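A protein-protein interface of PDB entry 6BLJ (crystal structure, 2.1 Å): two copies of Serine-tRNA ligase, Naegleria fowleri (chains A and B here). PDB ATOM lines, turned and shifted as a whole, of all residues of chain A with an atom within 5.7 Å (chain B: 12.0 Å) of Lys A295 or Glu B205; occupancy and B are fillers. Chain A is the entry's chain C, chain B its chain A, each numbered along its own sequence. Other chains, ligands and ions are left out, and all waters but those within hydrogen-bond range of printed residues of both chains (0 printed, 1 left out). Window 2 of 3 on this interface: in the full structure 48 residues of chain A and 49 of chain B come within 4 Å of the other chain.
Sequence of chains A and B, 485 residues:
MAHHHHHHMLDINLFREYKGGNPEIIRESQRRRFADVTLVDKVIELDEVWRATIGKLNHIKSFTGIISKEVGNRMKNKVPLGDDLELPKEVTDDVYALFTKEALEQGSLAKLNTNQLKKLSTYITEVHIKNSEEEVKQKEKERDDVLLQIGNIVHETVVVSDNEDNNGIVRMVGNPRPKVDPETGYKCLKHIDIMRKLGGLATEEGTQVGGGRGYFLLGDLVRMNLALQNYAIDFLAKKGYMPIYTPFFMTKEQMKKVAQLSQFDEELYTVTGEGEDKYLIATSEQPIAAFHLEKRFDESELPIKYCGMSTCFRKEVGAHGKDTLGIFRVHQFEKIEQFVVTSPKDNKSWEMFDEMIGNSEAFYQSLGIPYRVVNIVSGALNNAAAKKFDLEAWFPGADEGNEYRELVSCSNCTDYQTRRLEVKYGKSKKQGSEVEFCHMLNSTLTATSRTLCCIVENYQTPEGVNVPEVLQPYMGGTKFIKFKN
Of the 12 printed residues of chain A, 4 touch a printed residue of chain B.
Hydrophobic or aromatic side chains of chain A that line the printed part of chain B: Pro A247, Phe A291 and Leu A293.
Hydrophobic or aromatic side chains of chain B within 4 Å of the printed part of chain A: Ala B202 and Phe B216.
Along chain B the printed residues that touch a printed residue of chain A span positions 202 to 332.
Among the printed residues, Asp or Glu carboxylates within 4 Å of a Lys or Arg side-chain nitrogen of the other chain: Lys A295 with Glu B205 (2.6 Å).
Among the printed residues, merely in contact across the chains: Pro A247 with Tyr B215 (3.3 Å), Phe A291 with Glu B205 (3.4 Å), Leu A293 with Gln B208 (3.6 Å), Pro A247 with Gln B332 (3.7 Å), Pro A247 with Phe B216 (3.7 Å), Phe A291 with Phe B216 (3.7 Å) and Phe A291 with Ala B202 (3.9 Å).
Lys A295 touches just one residue of chain B: Glu B205.
Of chain A, only Phe A291 (3.4 Å) and Lys A295 (2.6 Å) come within 4 Å of Glu B205.
Of chain B, only Ala B202, Glu B205 and Phe B216 come within 4 Å of Phe A291.
Of the printed residues of chain B, Leu A293 touches Gln B208.
No residue of chain B comes within 4 Å of Arg A296.
Of the printed residues of chain A, Gln B208 touches Leu A293.
Of the printed residues of chain A, Ala B202 touches Phe A291 (3.9 Å).
Printed residues of chain A within 4 Å of Phe B216: Pro A247 (3.7 Å) and Phe A291 (3.7 Å).
Gly B212 touches none of the printed residues of chain A.
Gly B206 touches none of the printed residues of chain A.
The nearest printed residue of chain A that does not touch Tyr B215 is Phe A291 (7.3 Å).
The side-chain carboxylate of Glu B205 lies within salt-bridge range of the side-chain amino group of Lys A295 (2.6 Å).
The backbone NH of Ala B202 sits at hydrogen-bond distance from the backbone carbonyl oxygen of Phe B216, at 3.0 Å.
The backbone carbonyl oxygen of Gln B332 is in hydrogen-bond range of the side-chain hydroxyl of Tyr B215 (2.7 Å).
The backbone carbonyl oxygen (O) of Phe A291 sits at hydrogen-bond distance from the side-chain amino group (NZ) of Lys A295 (2.9 Å).
The backbone carbonyl oxygen (O) of Lys A295 lies within hydrogen-bond range of the backbone NH (N) of Lys A424 (3.0 Å).
No position is printed for both chains.
Of the 8 pairs that touch across the chains among the printed residues, none has its exchanged pair printed and touching as well.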
ATOM      1  N   PRO A 247      21.872  27.741  16.146  1.00  0.00           N
ATOM      2  CA  PRO A 247      23.161  27.055  16.304  1.00  0.00           C
ATOM      3  C   PRO A 247      24.239  27.859  15.600  1.00  0.00           C
ATOM      4  O   PRO A 247      23.988  28.473  14.559  1.00  0.00           O
ATOM      5  CB  PRO A 247      22.937  25.694  15.615  1.00  0.00           C
ATOM      6  CG  PRO A 247      21.438  25.491  15.653  1.00  0.00           C
ATOM      7  CD  PRO A 247      20.866  26.876  15.487  1.00  0.00           C
ATOM      8  N   PHE A 291      16.736  25.748   8.514  1.00  0.00           N
ATOM      9  CA  PHE A 291      15.560  25.575   9.362  1.00  0.00           C
ATOM     10  C   PHE A 291      14.317  25.229   8.548  1.00  0.00           C
ATOM     11  O   PHE A 291      13.405  24.566   9.055  1.00  0.00           O
ATOM     12  CB  PHE A 291      15.368  26.873  10.165  1.00  0.00           C
ATOM     13  CG  PHE A 291      14.241  26.852  11.178  1.00  0.00           C
ATOM     14  CD1 PHE A 291      14.501  26.554  12.517  1.00  0.00           C
ATOM     15  CD2 PHE A 291      12.949  27.216  10.819  1.00  0.00           C
ATOM     16  CE1 PHE A 291      13.473  26.558  13.471  1.00  0.00           C
ATOM     17  CE2 PHE A 291      11.913  27.242  11.764  1.00  0.00           C
ATOM     18  CZ  PHE A 291      12.177  26.910  13.093  1.00  0.00           C
ATOM     19  N   HIS A 292      14.271  25.650   7.283  1.00  0.00           N
ATOM     20  CA  HIS A 292      13.112  25.453   6.422  1.00  0.00           C
ATOM     21  C   HIS A 292      13.223  24.226   5.520  1.00  0.00           C
ATOM     22  O   HIS A 292      12.348  24.017   4.675  1.00  0.00           O
ATOM     23  CB  HIS A 292      12.886  26.711   5.590  1.00  0.00           C
ATOM     24  CG  HIS A 292      12.507  27.889   6.426  1.00  0.00           C
ATOM     25  ND1 HIS A 292      13.442  28.724   6.996  1.00  0.00           N
ATOM     26  CD2 HIS A 292      11.296  28.337   6.841  1.00  0.00           C
ATOM     27  CE1 HIS A 292      12.824  29.646   7.714  1.00  0.00           C
ATOM     28  NE2 HIS A 292      11.521  29.438   7.633  1.00  0.00           N
ATOM     29  N   LEU A 293      14.256  23.407   5.695  1.00  0.00           N
ATOM     30  CA  LEU A 293      14.446  22.211   4.881  1.00  0.00           C
ATOM     31  C   LEU A 293      13.158  21.406   4.760  1.00  0.00           C
ATOM     32  O   LEU A 293      12.528  21.066   5.767  1.00  0.00           O
ATOM     33  CB  LEU A 293      15.556  21.344   5.488  1.00  0.00           C
ATOM     34  CG  LEU A 293      15.803  20.045   4.709  1.00  0.00           C
ATOM     35  CD1 LEU A 293      16.384  20.338   3.334  1.00  0.00           C
ATOM     36  CD2 LEU A 293      16.713  19.100   5.488  1.00  0.00           C
ATOM     37  N   GLU A 294      12.750  21.157   3.512  1.00  0.00           N
ATOM     38  CA  GLU A 294      11.655  20.247   3.172  1.00  0.00           C
ATOM     39  C   GLU A 294      10.332  20.638   3.829  1.00  0.00           C
ATOM     40  O   GLU A 294       9.484  19.784   4.101  1.00  0.00           O
ATOM     41  CB  GLU A 294      12.029  18.795   3.497  1.00  0.00           C
ATOM     42  CG  GLU A 294      12.917  18.196   2.412  1.00  0.00           C
ATOM     43  CD  GLU A 294      13.818  17.093   2.910  1.00  0.00           C
ATOM     44  OE1 GLU A 294      13.586  16.600   4.030  1.00  0.00           O
ATOM     45  OE2 GLU A 294      14.767  16.729   2.176  1.00  0.00           O
ATOM     46  N   LYS A 295      10.128  21.926   4.065  1.00  0.00           N
ATOM     47  CA  LYS A 295       8.850  22.427   4.539  1.00  0.00           C
ATOM     48  C   LYS A 295       8.061  22.995   3.362  1.00  0.00           C
ATOM     49  O   LYS A 295       8.615  23.283   2.297  1.00  0.00           O
ATOM     50  CB  LYS A 295       9.053  23.482   5.637  1.00  0.00           C
ATOM     51  CG  LYS A 295       9.568  22.886   6.964  1.00  0.00           C
ATOM     52  CD  LYS A 295       9.711  23.938   8.044  1.00  0.00           C
ATOM     53  CE  LYS A 295      10.084  23.318   9.388  1.00  0.00           C
ATOM     54  NZ  LYS A 295      10.771  24.291  10.288  1.00  0.00           N
ATOM     55  N   ARG A 296       6.744  23.094   3.546  1.00  0.00           N
ATOM     56  CA  ARG A 296       5.827  23.618   2.538  1.00  0.00           C
ATOM     57  C   ARG A 296       4.933  24.678   3.167  1.00  0.00           C
ATOM     58  O   ARG A 296       4.473  24.512   4.300  1.00  0.00           O
ATOM     59  CB  ARG A 296       4.974  22.503   1.923  1.00  0.00           C
ATOM     60  N   PHE A 297       4.692  25.773   2.446  1.00  0.00           N
ATOM     61  CA  PHE A 297       3.894  26.867   2.983  1.00  0.00           C
ATOM     62  C   PHE A 297       2.820  27.318   1.998  1.00  0.00           C
ATOM     63  O   PHE A 297       3.059  27.382   0.787  1.00  0.00           O
ATOM     64  CB  PHE A 297       4.795  28.045   3.373  1.00  0.00           C
ATOM     65  CG  PHE A 297       5.824  27.686   4.414  1.00  0.00           C
ATOM     66  CD1 PHE A 297       5.459  27.517   5.737  1.00  0.00           C
ATOM     67  CD2 PHE A 297       7.147  27.484   4.056  1.00  0.00           C
ATOM     68  CE1 PHE A 297       6.394  27.177   6.688  1.00  0.00           C
ATOM     69  CE2 PHE A 297       8.095  27.139   5.007  1.00  0.00           C
ATOM     70  CZ  PHE A 297       7.719  26.986   6.321  1.00  0.00           C
ATOM     71  N   LEU A 421      16.696  23.437  -1.043  1.00  0.00           N
ATOM     72  CA  LEU A 421      16.204  23.076   0.276  1.00  0.00           C
ATOM     73  C   LEU A 421      14.802  22.485   0.236  1.00  0.00           C
ATOM     74  O   LEU A 421      14.291  22.062   1.281  1.00  0.00           O
ATOM     75  CB  LEU A 421      16.216  24.309   1.194  1.00  0.00           C
ATOM     76  CG  LEU A 421      17.581  24.852   1.625  1.00  0.00           C
ATOM     77  CD1 LEU A 421      17.461  26.280   2.144  1.00  0.00           C
ATOM     78  CD2 LEU A 421      18.206  23.933   2.687  1.00  0.00           C
ATOM     79  N   GLU A 422      14.170  22.447  -0.943  1.00  0.00           N
ATOM     80  CA  GLU A 422      12.802  21.947  -1.095  1.00  0.00           C
ATOM     81  C   GLU A 422      11.818  22.684  -0.189  1.00  0.00           C
ATOM     82  O   GLU A 422      11.038  22.074   0.550  1.00  0.00           O
ATOM     83  CB  GLU A 422      12.730  20.439  -0.853  1.00  0.00           C
ATOM     84  CG  GLU A 422      13.450  19.598  -1.879  1.00  0.00           C
ATOM     85  CD  GLU A 422      13.135  18.137  -1.704  1.00  0.00           C
ATOM     86  OE1 GLU A 422      11.934  17.798  -1.710  1.00  0.00           O
ATOM     87  OE2 GLU A 422      14.075  17.330  -1.561  1.00  0.00           O
ATOM     88  N   VAL A 423      11.868  24.014  -0.234  1.00  0.00           N
ATOM     89  CA  VAL A 423      10.890  24.851   0.470  1.00  0.00           C
ATOM     90  C   VAL A 423       9.777  25.128  -0.537  1.00  0.00           C
ATOM     91  O   VAL A 423       9.834  26.078  -1.325  1.00  0.00           O
ATOM     92  CB  VAL A 423      11.519  26.130   1.016  1.00  0.00           C
ATOM     93  CG1 VAL A 423      10.529  26.886   1.911  1.00  0.00           C
ATOM     94  CG2 VAL A 423      12.806  25.796   1.761  1.00  0.00           C
ATOM     95  N   LYS A 424       8.740  24.295  -0.498  1.00  0.00           N
ATOM     96  CA  LYS A 424       7.717  24.283  -1.530  1.00  0.00           C
ATOM     97  C   LYS A 424       6.600  25.272  -1.214  1.00  0.00           C
ATOM     98  O   LYS A 424       6.318  25.586  -0.053  1.00  0.00           O
ATOM     99  CB  LYS A 424       7.150  22.869  -1.690  1.00  0.00           C
ATOM    100  CG  LYS A 424       8.172  21.879  -2.240  1.00  0.00           C
ATOM    101  CD  LYS A 424       7.679  20.437  -2.183  1.00  0.00           C
ATOM    102  CE  LYS A 424       8.837  19.465  -2.414  1.00  0.00           C
ATOM    103  NZ  LYS A 424       8.402  18.072  -2.734  1.00  0.00           N
ATOM    104  N   ILE B 192      11.510  22.330  29.418  1.00  0.00           N
ATOM    105  CA  ILE B 192      11.380  22.049  27.981  1.00  0.00           C
ATOM    106  C   ILE B 192       9.917  22.146  27.534  1.00  0.00           C
ATOM    107  O   ILE B 192       9.617  22.694  26.464  1.00  0.00           O
ATOM    108  CB  ILE B 192      11.997  20.680  27.614  1.00  0.00           C
ATOM    109  CG1 ILE B 192      11.944  20.482  26.084  1.00  0.00           C
ATOM    110  CG2 ILE B 192      11.280  19.520  28.335  1.00  0.00           C
ATOM    111  CD1 ILE B 192      12.565  19.195  25.630  1.00  0.00           C
ATOM    112  N   MET B 195       8.900  25.912  27.477  1.00  0.00           N
ATOM    113  CA  MET B 195       9.452  26.658  26.345  1.00  0.00           C
ATOM    114  C   MET B 195       8.776  26.264  25.033  1.00  0.00           C
ATOM    115  O   MET B 195       8.525  27.117  24.173  1.00  0.00           O
ATOM    116  CB  MET B 195      10.965  26.442  26.250  1.00  0.00           C
ATOM    117  CG  MET B 195      11.727  27.049  27.417  1.00  0.00           C
ATOM    118  SD  MET B 195      13.517  26.909  27.215  1.00  0.00           S
ATOM    119  CE  MET B 195      14.053  27.837  28.655  1.00  0.00           C
ATOM    120  N   ARG B 196       8.461  24.982  24.866  1.00  0.00           N
ATOM    121  CA  ARG B 196       7.738  24.560  23.667  1.00  0.00           C
ATOM    122  C   ARG B 196       6.315  25.111  23.659  1.00  0.00           C
ATOM    123  O   ARG B 196       5.793  25.488  22.597  1.00  0.00           O
ATOM    124  CB  ARG B 196       7.720  23.032  23.560  1.00  0.00           C
ATOM    125  CG  ARG B 196       9.054  22.416  23.093  1.00  0.00           C
ATOM    126  CD  ARG B 196       8.975  20.884  23.026  1.00  0.00           C
ATOM    127  NE  ARG B 196      10.208  20.312  22.495  1.00  0.00           N
ATOM    128  CZ  ARG B 196      10.559  19.043  22.680  1.00  0.00           C
ATOM    129  NH1 ARG B 196       9.773  18.236  23.389  1.00  0.00           N
ATOM    130  NH2 ARG B 196      11.693  18.583  22.173  1.00  0.00           N
ATOM    131  N   GLY B 199       6.099  28.359  22.288  1.00  0.00           N
ATOM    132  CA  GLY B 199       6.552  28.488  20.913  1.00  0.00           C
ATOM    133  C   GLY B 199       7.958  29.039  20.798  1.00  0.00           C
ATOM    134  O   GLY B 199       8.304  29.629  19.775  1.00  0.00           O
ATOM    135  N   GLY B 200       8.787  28.855  21.822  1.00  0.00           N
ATOM    136  CA  GLY B 200      10.077  29.518  21.839  1.00  0.00           C
ATOM    137  C   GLY B 200      11.286  28.630  21.648  1.00  0.00           C
ATOM    138  O   GLY B 200      12.416  29.110  21.742  1.00  0.00           O
ATOM    139  N   LEU B 201      11.083  27.337  21.411  1.00  0.00           N
ATOM    140  CA  LEU B 201      12.199  26.402  21.384  1.00  0.00           C
ATOM    141  C   LEU B 201      11.979  25.372  20.298  1.00  0.00           C
ATOM    142  O   LEU B 201      10.947  24.689  20.289  1.00  0.00           O
ATOM    143  CB  LEU B 201      12.374  25.709  22.737  1.00  0.00           C
ATOM    144  CG  LEU B 201      13.469  24.645  22.840  1.00  0.00           C
ATOM    145  CD1 LEU B 201      14.820  25.279  22.575  1.00  0.00           C
ATOM    146  CD2 LEU B 201      13.452  23.942  24.216  1.00  0.00           C
ATOM    147  N   ALA B 202      12.965  25.228  19.415  1.00  0.00           N
ATOM    148  CA  ALA B 202      12.920  24.266  18.311  1.00  0.00           C
ATOM    149  C   ALA B 202      14.131  23.339  18.410  1.00  0.00           C
ATOM    150  O   ALA B 202      15.165  23.583  17.789  1.00  0.00           O
ATOM    151  CB  ALA B 202      12.884  24.996  16.973  1.00  0.00           C
ATOM    152  N   THR B 203      13.994  22.247  19.170  1.00  0.00           N
ATOM    153  CA  THR B 203      15.071  21.261  19.245  1.00  0.00           C
ATOM    154  C   THR B 203      15.117  20.367  18.013  1.00  0.00           C
ATOM    155  O   THR B 203      16.176  19.813  17.708  1.00  0.00           O
ATOM    156  CB  THR B 203      14.911  20.377  20.487  1.00  0.00           C
ATOM    157  OG1 THR B 203      13.698  19.626  20.353  1.00  0.00           O
ATOM    158  CG2 THR B 203      14.846  21.257  21.775  1.00  0.00           C
ATOM    159  N   GLU B 204      13.987  20.210  17.316  1.00  0.00           N
ATOM    160  CA  GLU B 204      13.925  19.366  16.125  1.00  0.00           C
ATOM    161  C   GLU B 204      14.758  19.954  14.981  1.00  0.00           C
ATOM    162  O   GLU B 204      15.697  19.321  14.497  1.00  0.00           O
ATOM    163  CB  GLU B 204      12.464  19.177  15.704  1.00  0.00           C
ATOM    164  CG  GLU B 204      11.597  18.367  16.692  1.00  0.00           C
ATOM    165  CD  GLU B 204      11.037  19.168  17.882  1.00  0.00           C
ATOM    166  OE1 GLU B 204      11.196  20.418  17.945  1.00  0.00           O
ATOM    167  OE2 GLU B 204      10.432  18.519  18.769  1.00  0.00           O
ATOM    168  N   GLU B 205      14.430  21.170  14.534  1.00  0.00           N
ATOM    169  CA  GLU B 205      15.294  21.852  13.571  1.00  0.00           C
ATOM    170  C   GLU B 205      16.694  22.074  14.146  1.00  0.00           C
ATOM    171  O   GLU B 205      17.686  21.987  13.420  1.00  0.00           O
ATOM    172  CB  GLU B 205      14.679  23.193  13.154  1.00  0.00           C
ATOM    173  CG  GLU B 205      13.396  23.075  12.328  1.00  0.00           C
ATOM    174  CD  GLU B 205      12.140  22.999  13.183  1.00  0.00           C
ATOM    175  OE1 GLU B 205      12.242  22.737  14.401  1.00  0.00           O
ATOM    176  OE2 GLU B 205      11.043  23.217  12.630  1.00  0.00           O
ATOM    177  N   GLY B 206      16.790  22.349  15.451  1.00  0.00           N
ATOM    178  CA  GLY B 206      18.092  22.573  16.066  1.00  0.00           C
ATOM    179  C   GLY B 206      19.038  21.391  15.912  1.00  0.00           C
ATOM    180  O   GLY B 206      20.216  21.552  15.575  1.00  0.00           O
ATOM    181  N   THR B 207      18.539  20.178  16.159  1.00  0.00           N
ATOM    182  CA  THR B 207      19.418  19.019  16.051  1.00  0.00           C
ATOM    183  C   THR B 207      19.629  18.629  14.596  1.00  0.00           C
ATOM    184  O   THR B 207      20.733  18.228  14.210  1.00  0.00           O
ATOM    185  CB  THR B 207      18.852  17.841  16.837  1.00  0.00           C
ATOM    186  OG1 THR B 207      17.567  17.516  16.314  1.00  0.00           O
ATOM    187  CG2 THR B 207      18.739  18.195  18.306  1.00  0.00           C
ATOM    188  N   GLN B 208      18.600  18.775  13.757  1.00  0.00           N
ATOM    189  CA  GLN B 208      18.810  18.569  12.327  1.00  0.00           C
ATOM    190  C   GLN B 208      19.927  19.475  11.805  1.00  0.00           C
ATOM    191  O   GLN B 208      20.823  19.020  11.092  1.00  0.00           O
ATOM    192  CB  GLN B 208      17.502  18.832  11.575  1.00  0.00           C
ATOM    193  CG  GLN B 208      17.596  18.738  10.056  1.00  0.00           C
ATOM    194  CD  GLN B 208      16.670  19.739   9.363  1.00  0.00           C
ATOM    195  OE1 GLN B 208      15.445  19.627   9.450  1.00  0.00           O
ATOM    196  NE2 GLN B 208      17.260  20.723   8.663  1.00  0.00           N
ATOM    197  N   VAL B 209      19.924  20.749  12.203  1.00  0.00           N
ATOM    198  CA  VAL B 209      20.887  21.704  11.653  1.00  0.00           C
ATOM    199  C   VAL B 209      22.253  21.589  12.338  1.00  0.00           C
ATOM    200  O   VAL B 209      23.295  21.608  11.673  1.00  0.00           O
ATOM    201  CB  VAL B 209      20.307  23.130  11.757  1.00  0.00           C
ATOM    202  CG1 VAL B 209      21.378  24.185  11.435  1.00  0.00           C
ATOM    203  CG2 VAL B 209      19.091  23.267  10.845  1.00  0.00           C
ATOM    204  N   GLY B 210      22.284  21.458  13.661  1.00  0.00           N
ATOM    205  CA  GLY B 210      23.540  21.589  14.393  1.00  0.00           C
ATOM    206  C   GLY B 210      24.076  20.346  15.090  1.00  0.00           C
ATOM    207  O   GLY B 210      25.102  20.416  15.787  1.00  0.00           O
ATOM    208  N   GLY B 211      23.392  19.214  14.939  1.00  0.00           N
ATOM    209  CA  GLY B 211      23.798  17.989  15.621  1.00  0.00           C
ATOM    210  C   GLY B 211      23.178  17.858  16.999  1.00  0.00           C
ATOM    211  O   GLY B 211      22.280  18.607  17.387  1.00  0.00           O
ATOM    212  N   GLY B 212      23.671  16.875  17.751  1.00  0.00           N
ATOM    213  CA  GLY B 212      23.076  16.577  19.047  1.00  0.00           C
ATOM    214  C   GLY B 212      23.069  17.796  19.959  1.00  0.00           C
ATOM    215  O   GLY B 212      23.980  18.629  19.925  1.00  0.00           O
ATOM    216  N   ARG B 213      21.999  17.917  20.753  1.00  0.00           N
ATOM    217  CA  ARG B 213      21.739  19.041  21.664  1.00  0.00           C
ATOM    218  C   ARG B 213      21.574  20.384  20.953  1.00  0.00           C
ATOM    219  O   ARG B 213      21.465  21.420  21.625  1.00  0.00           O
ATOM    220  CB  ARG B 213      22.836  19.182  22.734  1.00  0.00           C
ATOM    221  CG  ARG B 213      23.139  17.850  23.528  1.00  0.00           C
ATOM    222  CD  ARG B 213      24.057  18.124  24.778  1.00  0.00           C
ATOM    223  NE  ARG B 213      24.362  16.886  25.491  1.00  0.00           N
ATOM    224  CZ  ARG B 213      23.655  16.433  26.527  1.00  0.00           C
ATOM    225  NH1 ARG B 213      22.620  17.128  26.998  1.00  0.00           N
ATOM    226  NH2 ARG B 213      23.977  15.281  27.098  1.00  0.00           N
ATOM    227  N   GLY B 214      21.539  20.415  19.622  1.00  0.00           N
ATOM    228  CA  GLY B 214      21.355  21.689  18.924  1.00  0.00           C
ATOM    229  C   GLY B 214      19.964  22.268  19.134  1.00  0.00           C
ATOM    230  O   GLY B 214      18.971  21.546  19.249  1.00  0.00           O
ATOM    231  N   TYR B 215      19.880  23.603  19.164  1.00  0.00           N
ATOM    232  CA  TYR B 215      18.591  24.248  19.396  1.00  0.00           C
ATOM    233  C   TYR B 215      18.528  25.581  18.667  1.00  0.00           C
ATOM    234  O   TYR B 215      19.546  26.249  18.474  1.00  0.00           O
ATOM    235  CB  TYR B 215      18.319  24.468  20.909  1.00  0.00           C
ATOM    236  CG  TYR B 215      19.304  25.423  21.590  1.00  0.00           C
ATOM    237  CD1 TYR B 215      20.569  24.979  21.994  1.00  0.00           C
ATOM    238  CD2 TYR B 215      18.959  26.755  21.852  1.00  0.00           C
ATOM    239  CE1 TYR B 215      21.478  25.846  22.626  1.00  0.00           C
ATOM    240  CE2 TYR B 215      19.855  27.632  22.502  1.00  0.00           C
ATOM    241  CZ  TYR B 215      21.108  27.165  22.870  1.00  0.00           C
ATOM    242  OH  TYR B 215      22.003  28.000  23.487  1.00  0.00           O
ATOM    243  N   PHE B 216      17.316  25.959  18.255  1.00  0.00           N
ATOM    244  CA  PHE B 216      16.977  27.351  17.960  1.00  0.00           C
ATOM    245  C   PHE B 216      16.104  27.885  19.084  1.00  0.00           C
ATOM    246  O   PHE B 216      15.206  27.184  19.556  1.00  0.00           O
ATOM    247  CB  PHE B 216      16.180  27.522  16.655  1.00  0.00           C
ATOM    248  CG  PHE B 216      16.932  27.187  15.390  1.00  0.00           C
ATOM    249  CD1 PHE B 216      17.354  28.202  14.522  1.00  0.00           C
ATOM    250  CD2 PHE B 216      17.136  25.870  15.023  1.00  0.00           C
ATOM    251  CE1 PHE B 216      18.012  27.890  13.312  1.00  0.00           C
ATOM    252  CE2 PHE B 216      17.809  25.535  13.813  1.00  0.00           C
ATOM    253  CZ  PHE B 216      18.234  26.546  12.957  1.00  0.00           C
ATOM    254  N   LEU B 217      16.366  29.123  19.500  1.00  0.00           N
ATOM    255  CA  LEU B 217      15.507  29.849  20.426  1.00  0.00           C
ATOM    256  C   LEU B 217      14.750  30.913  19.636  1.00  0.00           C
ATOM    257  O   LEU B 217      15.318  31.548  18.736  1.00  0.00           O
ATOM    258  CB  LEU B 217      16.334  30.486  21.556  1.00  0.00           C
ATOM    259  CG  LEU B 217      15.707  30.642  22.949  1.00  0.00           C
ATOM    260  CD1 LEU B 217      15.461  29.276  23.583  1.00  0.00           C
ATOM    261  CD2 LEU B 217      16.577  31.511  23.866  1.00  0.00           C
ATOM    262  N   LEU B 218      13.449  31.086  19.939  1.00  0.00           N
ATOM    263  CA  LEU B 218      12.599  32.016  19.181  1.00  0.00           C
ATOM    264  C   LEU B 218      11.818  32.986  20.071  1.00  0.00           C
ATOM    265  O   LEU B 218      11.385  32.643  21.174  1.00  0.00           O
ATOM    266  CB  LEU B 218      11.571  31.273  18.297  1.00  0.00           C
ATOM    267  CG  LEU B 218      12.128  30.378  17.170  1.00  0.00           C
ATOM    268  CD1 LEU B 218      12.439  29.010  17.721  1.00  0.00           C
ATOM    269  CD2 LEU B 218      11.174  30.280  15.991  1.00  0.00           C
ATOM    270  N   GLY B 326      15.930  19.709  26.333  1.00  0.00           N
ATOM    271  CA  GLY B 326      15.907  21.165  26.395  1.00  0.00           C
ATOM    272  C   GLY B 326      17.296  21.787  26.393  1.00  0.00           C
ATOM    273  O   GLY B 326      18.252  21.230  25.868  1.00  0.00           O
ATOM    274  N   ILE B 327      17.410  22.959  27.006  1.00  0.00           N
ATOM    275  CA  ILE B 327      18.640  23.741  26.892  1.00  0.00           C
ATOM    276  C   ILE B 327      19.356  23.878  28.243  1.00  0.00           C
ATOM    277  O   ILE B 327      20.140  24.813  28.448  1.00  0.00           O
ATOM    278  CB  ILE B 327      18.355  25.105  26.238  1.00  0.00           C
ATOM    279  CG1 ILE B 327      17.495  26.012  27.135  1.00  0.00           C
ATOM    280  CG2 ILE B 327      17.638  24.874  24.894  1.00  0.00           C
ATOM    281  CD1 ILE B 327      17.219  27.392  26.466  1.00  0.00           C
ATOM    282  N   GLN B 332      26.444  24.856  23.370  1.00  0.00           N
ATOM    283  CA  GLN B 332      26.607  26.267  23.026  1.00  0.00           C
ATOM    284  C   GLN B 332      25.702  27.108  23.917  1.00  0.00           C
ATOM    285  O   GLN B 332      24.477  26.933  23.895  1.00  0.00           O
ATOM    286  CB  GLN B 332      26.265  26.484  21.544  1.00  0.00           C
ATOM    287  CG  GLN B 332      26.260  27.921  21.061  1.00  0.00           C
ATOM    288  CD  GLN B 332      25.641  28.033  19.666  1.00  0.00           C
ATOM    289  OE1 GLN B 332      25.973  27.267  18.763  1.00  0.00           O
ATOM    290  NE2 GLN B 332      24.713  28.959  19.503  1.00  0.00           N
ATOM    291  N   ASN B 485       0.395  27.151  22.864  1.00  0.00           N
ATOM    292  CA  ASN B 485      -0.229  25.857  22.659  1.00  0.00           C
ATOM    293  C   ASN B 485      -0.203  25.053  23.956  1.00  0.00           C
ATOM    294  O   ASN B 485      -0.731  23.942  24.019  1.00  0.00           O
ATOM    295  CB  ASN B 485       0.472  25.109  21.521  1.00  0.00           C
ATOM    296  CG  ASN B 485       1.926  24.820  21.825  1.00  0.00           C
ATOM    297  OD1 ASN B 485       2.232  23.978  22.664  1.00  0.00           O
ATOM    298  ND2 ASN B 485       2.834  25.524  21.151  1.00  0.00           N
ATOM    299  OXT ASN B 485       0.351  25.494  24.970  1.00  0.00           O
